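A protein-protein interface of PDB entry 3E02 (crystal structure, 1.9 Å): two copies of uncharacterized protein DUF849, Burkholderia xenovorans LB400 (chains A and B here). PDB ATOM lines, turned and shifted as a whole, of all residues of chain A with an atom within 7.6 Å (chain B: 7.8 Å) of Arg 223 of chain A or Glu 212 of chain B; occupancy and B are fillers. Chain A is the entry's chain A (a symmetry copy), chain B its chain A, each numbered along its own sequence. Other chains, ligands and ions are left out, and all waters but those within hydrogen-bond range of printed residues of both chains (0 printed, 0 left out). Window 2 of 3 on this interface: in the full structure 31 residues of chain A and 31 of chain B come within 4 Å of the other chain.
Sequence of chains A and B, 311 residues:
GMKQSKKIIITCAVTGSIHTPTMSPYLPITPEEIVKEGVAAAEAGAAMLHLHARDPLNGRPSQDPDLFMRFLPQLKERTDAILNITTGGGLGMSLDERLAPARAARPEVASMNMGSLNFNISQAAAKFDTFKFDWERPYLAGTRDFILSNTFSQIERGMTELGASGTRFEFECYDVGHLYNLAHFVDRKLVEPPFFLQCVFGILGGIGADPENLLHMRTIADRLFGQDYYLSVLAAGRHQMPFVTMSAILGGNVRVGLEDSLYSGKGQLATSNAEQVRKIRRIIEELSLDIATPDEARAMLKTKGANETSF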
ATOM      1  N   MET A   2      11.809  15.590  13.380  1.00  0.00           N
ATOM      2  CA  MET A   2      11.459  14.252  12.819  1.00  0.00           C
ATOM      3  C   MET A   2      10.137  14.305  12.061  1.00  0.00           C
ATOM      4  O   MET A   2       9.154  14.825  12.597  1.00  0.00           O
ATOM      5  CB  MET A   2      11.281  13.238  13.960  1.00  0.00           C
ATOM      6  CG  MET A   2      11.217  11.772  13.517  1.00  0.00           C
ATOM      7  SD  MET A   2      10.406  10.652  14.880  1.00  0.00           S
ATOM      8  CE  MET A   2       8.587  11.429  14.829  1.00  0.00           C
ATOM      9  N   TYR A 180      26.228  13.713  14.346  1.00  0.00           N
ATOM     10  CA  TYR A 180      27.064  14.855  14.022  1.00  0.00           C
ATOM     11  C   TYR A 180      27.893  14.610  12.759  1.00  0.00           C
ATOM     12  O   TYR A 180      28.092  15.538  11.964  1.00  0.00           O
ATOM     13  CB  TYR A 180      27.948  15.245  15.208  1.00  0.00           C
ATOM     14  CG  TYR A 180      27.130  15.809  16.340  1.00  0.00           C
ATOM     15  CD1 TYR A 180      26.806  17.159  16.384  1.00  0.00           C
ATOM     16  CD2 TYR A 180      26.653  14.981  17.368  1.00  0.00           C
ATOM     17  CE1 TYR A 180      26.023  17.686  17.446  1.00  0.00           C
ATOM     18  CE2 TYR A 180      25.869  15.488  18.409  1.00  0.00           C
ATOM     19  CZ  TYR A 180      25.575  16.837  18.454  1.00  0.00           C
ATOM     20  OH  TYR A 180      24.820  17.311  19.493  1.00  0.00           O
ATOM     21  N   HIS A 216      17.264  10.359  23.507  1.00  0.00           N
ATOM     22  CA  HIS A 216      18.341  11.334  23.378  1.00  0.00           C
ATOM     23  C   HIS A 216      18.756  11.518  21.918  1.00  0.00           C
ATOM     24  O   HIS A 216      18.888  12.645  21.465  1.00  0.00           O
ATOM     25  CB  HIS A 216      19.558  10.990  24.240  1.00  0.00           C
ATOM     26  CG  HIS A 216      20.663  11.996  24.126  1.00  0.00           C
ATOM     27  ND1 HIS A 216      20.574  13.264  24.661  1.00  0.00           N
ATOM     28  CD2 HIS A 216      21.866  11.930  23.509  1.00  0.00           C
ATOM     29  CE1 HIS A 216      21.682  13.931  24.384  1.00  0.00           C
ATOM     30  NE2 HIS A 216      22.484  13.140  23.691  1.00  0.00           N
ATOM     31  N   MET A 217      18.962  10.407  21.206  1.00  0.00           N
ATOM     32  CA  MET A 217      19.317  10.466  19.787  1.00  0.00           C
ATOM     33  C   MET A 217      18.228  11.154  18.954  1.00  0.00           C
ATOM     34  O   MET A 217      18.556  11.925  18.045  1.00  0.00           O
ATOM     35  CB  MET A 217      19.664   9.078  19.252  1.00  0.00           C
ATOM     36  CG  MET A 217      21.016   8.580  19.755  1.00  0.00           C
ATOM     37  SD  MET A 217      21.491   6.876  19.006  1.00  0.00           S
ATOM     38  CE  MET A 217      22.157   7.525  17.306  1.00  0.00           C
ATOM     39  N   ARG A 218      16.949  10.939  19.290  1.00  0.00           N
ATOM     40  CA  ARG A 218      15.867  11.635  18.581  1.00  0.00           C
ATOM     41  C   ARG A 218      15.939  13.154  18.836  1.00  0.00           C
ATOM     42  O   ARG A 218      15.745  13.947  17.909  1.00  0.00           O
ATOM     43  CB  ARG A 218      14.475  11.102  18.931  1.00  0.00           C
ATOM     44  CG  ARG A 218      13.471  11.653  17.920  1.00  0.00           C
ATOM     45  CD  ARG A 218      12.086  11.322  18.139  1.00  0.00           C
ATOM     46  NE  ARG A 218      11.567  11.754  19.437  1.00  0.00           N
ATOM     47  CZ  ARG A 218      10.274  11.794  19.736  1.00  0.00           C
ATOM     48  NH1 ARG A 218       9.354  11.508  18.817  1.00  0.00           N
ATOM     49  NH2 ARG A 218       9.900  12.172  20.948  1.00  0.00           N
ATOM     50  N   THR A 219      16.230  13.553  20.080  1.00  0.00           N
ATOM     51  CA  THR A 219      16.368  14.973  20.444  1.00  0.00           C
ATOM     52  C   THR A 219      17.497  15.661  19.676  1.00  0.00           C
ATOM     53  O   THR A 219      17.321  16.776  19.153  1.00  0.00           O
ATOM     54  CB  THR A 219      16.580  15.131  21.970  1.00  0.00           C
ATOM     55  OG1 THR A 219      15.420  14.618  22.619  1.00  0.00           O
ATOM     56  CG2 THR A 219      16.779  16.570  22.379  1.00  0.00           C
ATOM     57  N   ILE A 220      18.630  14.979  19.589  1.00  0.00           N
ATOM     58  CA  ILE A 220      19.789  15.481  18.849  1.00  0.00           C
ATOM     59  C   ILE A 220      19.504  15.529  17.347  1.00  0.00           C
ATOM     60  O   ILE A 220      19.814  16.539  16.702  1.00  0.00           O
ATOM     61  CB  ILE A 220      21.064  14.655  19.168  1.00  0.00           C
ATOM     62  CG1 ILE A 220      21.446  14.823  20.654  1.00  0.00           C
ATOM     63  CG2 ILE A 220      22.225  15.062  18.266  1.00  0.00           C
ATOM     64  CD1 ILE A 220      21.656  16.280  21.140  1.00  0.00           C
ATOM     65  N   ALA A 221      18.902  14.467  16.803  1.00  0.00           N
ATOM     66  CA  ALA A 221      18.523  14.417  15.370  1.00  0.00           C
ATOM     67  C   ALA A 221      17.538  15.541  15.029  1.00  0.00           C
ATOM     68  O   ALA A 221      17.667  16.171  13.974  1.00  0.00           O
ATOM     69  CB  ALA A 221      17.945  13.064  14.995  1.00  0.00           C
ATOM     70  N   ASP A 222      16.580  15.809  15.918  1.00  0.00           N
ATOM     71  CA  ASP A 222      15.656  16.943  15.722  1.00  0.00           C
ATOM     72  C   ASP A 222      16.403  18.273  15.674  1.00  0.00           C
ATOM     73  O   ASP A 222      16.089  19.125  14.845  1.00  0.00           O
ATOM     74  CB  ASP A 222      14.581  17.022  16.805  1.00  0.00           C
ATOM     75  CG  ASP A 222      13.504  15.947  16.678  1.00  0.00           C
ATOM     76  OD1 ASP A 222      13.413  15.264  15.650  1.00  0.00           O
ATOM     77  OD2 ASP A 222      12.729  15.792  17.641  1.00  0.00           O
ATOM     78  N   ARG A 223      17.385  18.441  16.551  1.00  0.00           N
ATOM     79  CA  ARG A 223      18.205  19.654  16.579  1.00  0.00           C
ATOM     80  C   ARG A 223      19.044  19.816  15.317  1.00  0.00           C
ATOM     81  O   ARG A 223      19.135  20.915  14.786  1.00  0.00           O
ATOM     82  CB  ARG A 223      19.106  19.664  17.818  1.00  0.00           C
ATOM     83  CG  ARG A 223      20.201  20.726  17.813  1.00  0.00           C
ATOM     84  CD  ARG A 223      20.727  20.993  19.200  1.00  0.00           C
ATOM     85  NE  ARG A 223      19.676  21.588  20.031  1.00  0.00           N
ATOM     86  CZ  ARG A 223      19.850  22.122  21.238  1.00  0.00           C
ATOM     87  NH1 ARG A 223      21.061  22.188  21.817  1.00  0.00           N
ATOM     88  NH2 ARG A 223      18.781  22.631  21.864  1.00  0.00           N
ATOM     89  N   LEU A 224      19.658  18.731  14.859  1.00  0.00           N
ATOM     90  CA  LEU A 224      20.513  18.757  13.666  1.00  0.00           C
ATOM     91  C   LEU A 224      19.761  18.783  12.324  1.00  0.00           C
ATOM     92  O   LEU A 224      20.213  19.447  11.397  1.00  0.00           O
ATOM     93  CB  LEU A 224      21.465  17.547  13.683  1.00  0.00           C
ATOM     94  CG  LEU A 224      22.497  17.493  14.816  1.00  0.00           C
ATOM     95  CD1 LEU A 224      23.238  16.121  14.885  1.00  0.00           C
ATOM     96  CD2 LEU A 224      23.496  18.626  14.687  1.00  0.00           C
ATOM     97  N   PHE A 225      18.649  18.052  12.225  1.00  0.00           N
ATOM     98  CA  PHE A 225      17.911  17.836  10.951  1.00  0.00           C
ATOM     99  C   PHE A 225      16.441  18.246  10.893  1.00  0.00           C
ATOM    100  O   PHE A 225      15.832  18.148   9.815  1.00  0.00           O
ATOM    101  CB  PHE A 225      17.964  16.345  10.595  1.00  0.00           C
ATOM    102  CG  PHE A 225      19.326  15.746  10.727  1.00  0.00           C
ATOM    103  CD1 PHE A 225      20.350  16.132   9.866  1.00  0.00           C
ATOM    104  CD2 PHE A 225      19.596  14.791  11.705  1.00  0.00           C
ATOM    105  CE1 PHE A 225      21.619  15.598   9.987  1.00  0.00           C
ATOM    106  CE2 PHE A 225      20.869  14.248  11.827  1.00  0.00           C
ATOM    107  CZ  PHE A 225      21.881  14.654  10.969  1.00  0.00           C
ATOM    108  N   GLY A 226      15.861  18.663  12.015  1.00  0.00           N
ATOM    109  CA  GLY A 226      14.453  19.112  12.067  1.00  0.00           C
ATOM    110  C   GLY A 226      13.460  18.141  11.430  1.00  0.00           C
ATOM    111  O   GLY A 226      13.395  16.968  11.811  1.00  0.00           O
ATOM    112  N   TYR A 229      14.158  14.271   8.370  1.00  0.00           N
ATOM    113  CA  TYR A 229      14.550  12.871   8.582  1.00  0.00           C
ATOM    114  C   TYR A 229      13.435  11.939   9.060  1.00  0.00           C
ATOM    115  O   TYR A 229      12.464  12.375   9.670  1.00  0.00           O
ATOM    116  CB  TYR A 229      15.745  12.786   9.557  1.00  0.00           C
ATOM    117  CG  TYR A 229      15.400  12.817  11.025  1.00  0.00           C
ATOM    118  CD1 TYR A 229      15.188  14.025  11.694  1.00  0.00           C
ATOM    119  CD2 TYR A 229      15.291  11.629  11.763  1.00  0.00           C
ATOM    120  CE1 TYR A 229      14.861  14.059  13.043  1.00  0.00           C
ATOM    121  CE2 TYR A 229      14.970  11.648  13.114  1.00  0.00           C
ATOM    122  CZ  TYR A 229      14.760  12.861  13.756  1.00  0.00           C
ATOM    123  OH  TYR A 229      14.441  12.866  15.084  1.00  0.00           O
ATOM    124  N   PHE B 201      34.010  16.904  24.357  1.00  0.00           N
ATOM    125  CA  PHE B 201      32.993  17.456  23.449  1.00  0.00           C
ATOM    126  C   PHE B 201      33.563  18.330  22.343  1.00  0.00           C
ATOM    127  O   PHE B 201      34.524  19.059  22.555  1.00  0.00           O
ATOM    128  CB  PHE B 201      31.987  18.281  24.245  1.00  0.00           C
ATOM    129  CG  PHE B 201      31.319  17.506  25.328  1.00  0.00           C
ATOM    130  CD1 PHE B 201      31.892  17.437  26.597  1.00  0.00           C
ATOM    131  CD2 PHE B 201      30.152  16.785  25.077  1.00  0.00           C
ATOM    132  CE1 PHE B 201      31.313  16.661  27.598  1.00  0.00           C
ATOM    133  CE2 PHE B 201      29.551  16.020  26.087  1.00  0.00           C
ATOM    134  CZ  PHE B 201      30.138  15.963  27.343  1.00  0.00           C
ATOM    135  N   ILE B 207      31.225  13.156  20.047  1.00  0.00           N
ATOM    136  CA  ILE B 207      29.950  13.773  20.427  1.00  0.00           C
ATOM    137  C   ILE B 207      30.064  15.312  20.332  1.00  0.00           C
ATOM    138  O   ILE B 207      31.105  15.884  20.631  1.00  0.00           O
ATOM    139  CB  ILE B 207      29.489  13.257  21.803  1.00  0.00           C
ATOM    140  CG1 ILE B 207      27.978  13.439  21.995  1.00  0.00           C
ATOM    141  CG2 ILE B 207      30.327  13.896  22.933  1.00  0.00           C
ATOM    142  CD1 ILE B 207      27.434  12.656  23.202  1.00  0.00           C
ATOM    143  N   GLY B 208      29.001  15.949  19.840  1.00  0.00           N
ATOM    144  CA  GLY B 208      28.977  17.386  19.637  1.00  0.00           C
ATOM    145  C   GLY B 208      28.900  18.198  20.906  1.00  0.00           C
ATOM    146  O   GLY B 208      28.443  17.718  21.947  1.00  0.00           O
ATOM    147  N   ALA B 209      29.281  19.461  20.801  1.00  0.00           N
ATOM    148  CA  ALA B 209      29.265  20.374  21.951  1.00  0.00           C
ATOM    149  C   ALA B 209      27.896  21.034  22.127  1.00  0.00           C
ATOM    150  O   ALA B 209      27.770  22.250  22.044  1.00  0.00           O
ATOM    151  CB  ALA B 209      30.383  21.410  21.825  1.00  0.00           C
ATOM    152  N   ASP B 210      26.876  20.210  22.365  1.00  0.00           N
ATOM    153  CA  ASP B 210      25.521  20.641  22.715  1.00  0.00           C
ATOM    154  C   ASP B 210      25.363  20.257  24.199  1.00  0.00           C
ATOM    155  O   ASP B 210      25.661  19.111  24.562  1.00  0.00           O
ATOM    156  CB  ASP B 210      24.458  19.959  21.863  1.00  0.00           C
ATOM    157  CG  ASP B 210      24.373  20.549  20.449  1.00  0.00           C
ATOM    158  OD1 ASP B 210      24.159  21.766  20.328  1.00  0.00           O
ATOM    159  OD2 ASP B 210      24.487  19.795  19.460  1.00  0.00           O
ATOM    160  N   PRO B 211      24.921  21.198  25.070  1.00  0.00           N
ATOM    161  CA  PRO B 211      24.756  20.927  26.516  1.00  0.00           C
ATOM    162  C   PRO B 211      24.021  19.655  26.904  1.00  0.00           C
ATOM    163  O   PRO B 211      24.419  19.005  27.873  1.00  0.00           O
ATOM    164  CB  PRO B 211      23.932  22.135  26.984  1.00  0.00           C
ATOM    165  CG  PRO B 211      24.482  23.218  26.183  1.00  0.00           C
ATOM    166  CD  PRO B 211      24.536  22.602  24.788  1.00  0.00           C
ATOM    167  N   GLU B 212      22.969  19.313  26.156  1.00  0.00           N
ATOM    168  CA  GLU B 212      22.199  18.096  26.393  1.00  0.00           C
ATOM    169  C   GLU B 212      23.095  16.843  26.419  1.00  0.00           C
ATOM    170  O   GLU B 212      22.804  15.889  27.145  1.00  0.00           O
ATOM    171  CB  GLU B 212      21.117  17.860  25.334  1.00  0.00           C
ATOM    172  CG  GLU B 212      20.004  18.880  25.275  1.00  0.00           C
ATOM    173  CD  GLU B 212      20.295  20.074  24.373  1.00  0.00           C
ATOM    174  OE1 GLU B 212      21.481  20.354  24.022  1.00  0.00           O
ATOM    175  OE2 GLU B 212      19.299  20.739  24.030  1.00  0.00           O
ATOM    176  N   ASN B 213      24.158  16.844  25.606  1.00  0.00           N
ATOM    177  CA  ASN B 213      25.096  15.711  25.562  1.00  0.00           C
ATOM    178  C   ASN B 213      25.852  15.504  26.875  1.00  0.00           C
ATOM    179  O   ASN B 213      26.099  14.364  27.246  1.00  0.00           O
ATOM    180  CB  ASN B 213      26.068  15.839  24.367  1.00  0.00           C
ATOM    181  CG  ASN B 213      25.360  15.704  23.025  1.00  0.00           C
ATOM    182  OD1 ASN B 213      24.390  14.953  22.899  1.00  0.00           O
ATOM    183  ND2 ASN B 213      25.854  16.415  22.006  1.00  0.00           N
ATOM    184  N   LEU B 214      26.200  16.592  27.572  1.00  0.00           N
ATOM    185  CA  LEU B 214      26.879  16.486  28.861  1.00  0.00           C
ATOM    186  C   LEU B 214      25.958  15.903  29.927  1.00  0.00           C
ATOM    187  O   LEU B 214      26.343  14.976  30.640  1.00  0.00           O
ATOM    188  CB  LEU B 214      27.440  17.834  29.321  1.00  0.00           C
ATOM    189  CG  LEU B 214      28.075  17.912  30.715  1.00  0.00           C
ATOM    190  CD1 LEU B 214      29.131  16.846  30.934  1.00  0.00           C
ATOM    191  CD2 LEU B 214      28.628  19.335  30.878  1.00  0.00           C
ATOM    192  N   LEU B 215      24.752  16.461  30.045  1.00  0.00           N
ATOM    193  CA  LEU B 215      23.795  15.952  31.034  1.00  0.00           C
ATOM    194  C   LEU B 215      23.419  14.509  30.730  1.00  0.00           C
ATOM    195  O   LEU B 215      23.259  13.742  31.648  1.00  0.00           O
ATOM    196  CB  LEU B 215      22.548  16.829  31.189  1.00  0.00           C
ATOM    197  CG  LEU B 215      22.740  18.098  32.037  1.00  0.00           C
ATOM    198  CD1 LEU B 215      23.462  19.186  31.243  1.00  0.00           C
ATOM    199  CD2 LEU B 215      21.391  18.608  32.553  1.00  0.00           C
ATOM    200  N   HIS B 216      23.311  14.154  29.448  1.00  0.00           N
ATOM    201  CA  HIS B 216      22.994  12.786  29.056  1.00  0.00           C
ATOM    202  C   HIS B 216      24.098  11.815  29.472  1.00  0.00           C
ATOM    203  O   HIS B 216      23.804  10.771  30.037  1.00  0.00           O
ATOM    204  CB  HIS B 216      22.699  12.652  27.560  1.00  0.00           C
ATOM    205  CG  HIS B 216      22.355  11.252  27.152  1.00  0.00           C
ATOM    206  ND1 HIS B 216      21.164  10.646  27.496  1.00  0.00           N
ATOM    207  CD2 HIS B 216      23.061  10.328  26.458  1.00  0.00           C
ATOM    208  CE1 HIS B 216      21.151   9.413  27.021  1.00  0.00           C
ATOM    209  NE2 HIS B 216      22.289   9.198  26.381  1.00  0.00           N
ATOM    210  N   MET B 217      25.352  12.168  29.181  1.00  0.00           N
ATOM    211  CA  MET B 217      26.491  11.336  29.575  1.00  0.00           C
ATOM    212  C   MET B 217      26.576  11.167  31.098  1.00  0.00           C
ATOM    213  O   MET B 217      26.883  10.068  31.570  1.00  0.00           O
ATOM    214  CB  MET B 217      27.791  11.870  28.978  1.00  0.00           C
ATOM    215  CG  MET B 217      27.893  11.614  27.477  1.00  0.00           C
ATOM    216  SD  MET B 217      29.569  12.203  26.748  1.00  0.00           S
ATOM    217  CE  MET B 217      30.624  10.662  27.267  1.00  0.00           C
ATOM    218  N   ARG B 218      26.248  12.216  31.865  1.00  0.00           N
ATOM    219  CA  ARG B 218      26.231  12.090  33.329  1.00  0.00           C
ATOM    220  C   ARG B 218      25.136  11.101  33.776  1.00  0.00           C
ATOM    221  O   ARG B 218      25.366  10.289  34.679  1.00  0.00           O
ATOM    222  CB  ARG B 218      26.065  13.430  34.049  1.00  0.00           C
ATOM    223  CG  ARG B 218      26.385  13.234  35.530  1.00  0.00           C
ATOM    224  CD  ARG B 218      26.202  14.377  36.387  1.00  0.00           C
ATOM    225  NE  ARG B 218      24.843  14.918  36.379  1.00  0.00           N
ATOM    226  CZ  ARG B 218      24.390  15.782  37.280  1.00  0.00           C
ATOM    227  NH1 ARG B 218      25.149  16.153  38.310  1.00  0.00           N
ATOM    228  NH2 ARG B 218      23.153  16.240  37.174  1.00  0.00           N
ATOM    229  N   THR B 219      23.960  11.160  33.140  1.00  0.00           N
ATOM    230  CA  THR B 219      22.847  10.245  33.445  1.00  0.00           C
ATOM    231  C   THR B 219      23.212   8.783  33.188  1.00  0.00           C
ATOM    232  O   THR B 219      22.935   7.903  34.022  1.00  0.00           O
ATOM    233  CB  THR B 219      21.581  10.634  32.645  1.00  0.00           C
ATOM    234  OG1 THR B 219      21.201  11.945  33.053  1.00  0.00           O
ATOM    235  CG2 THR B 219      20.431   9.688  32.888  1.00  0.00           C
ATOM    236  N   PHE B 243      31.354  24.757  28.649  1.00  0.00           N
ATOM    237  CA  PHE B 243      31.301  23.330  29.046  1.00  0.00           C
ATOM    238  C   PHE B 243      31.922  23.029  30.402  1.00  0.00           C
ATOM    239  O   PHE B 243      31.314  22.311  31.180  1.00  0.00           O
ATOM    240  CB  PHE B 243      31.844  22.393  27.964  1.00  0.00           C
ATOM    241  CG  PHE B 243      30.779  21.935  27.035  1.00  0.00           C
ATOM    242  CD1 PHE B 243      30.189  22.824  26.138  1.00  0.00           C
ATOM    243  CD2 PHE B 243      30.272  20.646  27.137  1.00  0.00           C
ATOM    244  CE1 PHE B 243      29.146  22.408  25.305  1.00  0.00           C
ATOM    245  CE2 PHE B 243      29.236  20.226  26.315  1.00  0.00           C
ATOM    246  CZ  PHE B 243      28.668  21.100  25.416  1.00  0.00           C
ATOM    247  N   MET B 246      29.641  24.422  33.056  1.00  0.00           N
ATOM    248  CA  MET B 246      28.524  23.462  33.187  1.00  0.00           C
ATOM    249  C   MET B 246      28.971  22.285  34.085  1.00  0.00           C
ATOM    250  O   MET B 246      28.250  21.883  35.007  1.00  0.00           O
ATOM    251  CB  MET B 246      28.081  23.013  31.773  1.00  0.00           C
ATOM    252  CG  MET B 246      26.721  22.355  31.583  1.00  0.00           C
ATOM    253  SD  MET B 246      26.050  22.969  29.767  1.00  0.00           S
ATOM    254  CE  MET B 246      27.472  22.498  28.729  1.00  0.00           C
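The backbone carbonyl oxygen of Gly 208 of chain B sits at hydrogen-bond distance from the side-chain amide nitrogen of Asn 213 of chain B (2.9 Å).
Arg 223 of chain A touches just these residues of chain B: Asp 210 (3.5 Å) and Glu 212 (2.9 Å).
Of chain A, only His 216 (3.6 Å) and Arg 223 (2.9 Å) come within 4 Å of Glu 212 of chain B.
Of the printed residues of chain A, His 216 of chain B touches His 216.
Printed residues of chain B within 4 Å of Tyr 180 of chain A: Gly 208, Asp 210 and Asn 213.
Of the printed residues of chain A, Asn 213 of chain B touches Tyr 180, His 216 and Ile 220.
The nearest printed residue of chain B that does not touch His 216 of chain A is Ile 207 of chain B (5.0 Å).
Of the 16 printed residues of chain B, 5 touch a printed residue of chain A.
Hydrophobic or aromatic side chains of chain B that line the printed part of chain A: His 216.
Of the 14 printed residues of chain A, 4 touch a printed residue of chain B.
Printed residues of chain A that touch a printed residue of chain B: Tyr 180, His 216, Ile 220 and Arg 223.
Hydrophobic or aromatic side chains of chain A within 4 Å of the printed part of chain B: Tyr 180, His 216 and Ile 220.
His 216 of chain B touches its own counterpart, His 216 of chain A.
Of the 9 pairs that touch across the chains among the printed residues, 1 has its exchanged pair printed and touching as well.
OD2 of Asp 210 of chain B lies within hydrogen-bond range of OH of Tyr 180 of chain A (2.5 Å).
The guanidinium group (NH1) of Arg 223 of chain A lies within salt-bridge range of the side-chain carboxylate (OD1) of Asp 210 of chain B, at 3.5 Å.
OE1 of Glu 212 of chain B is in salt-bridge range of NH1 of Arg 223 of chain A, 2.9 Å away.
The side-chain amide nitrogen (ND2) of Asn 213 of chain B lies within hydrogen-bond range of the side-chain hydroxyl (OH) of Tyr 180 of chain A (2.9 Å).
OD1 of Asn 213 of chain B lies within hydrogen-bond range of NE2 of His 216 of chain A, 2.7 Å away.
Tyr 180 of chain A touches Gly 208 of chain B.
His 216 of chain A touches Glu 212 of chain B (CE1 to O, 3.6 Å).
CG of His 216 of chain B touches CG of His 216 of chain A (3.5 Å).
Ile 220 of chain A touches Asn 213 of chain B (CD1 to OD1, 3.5 Å).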
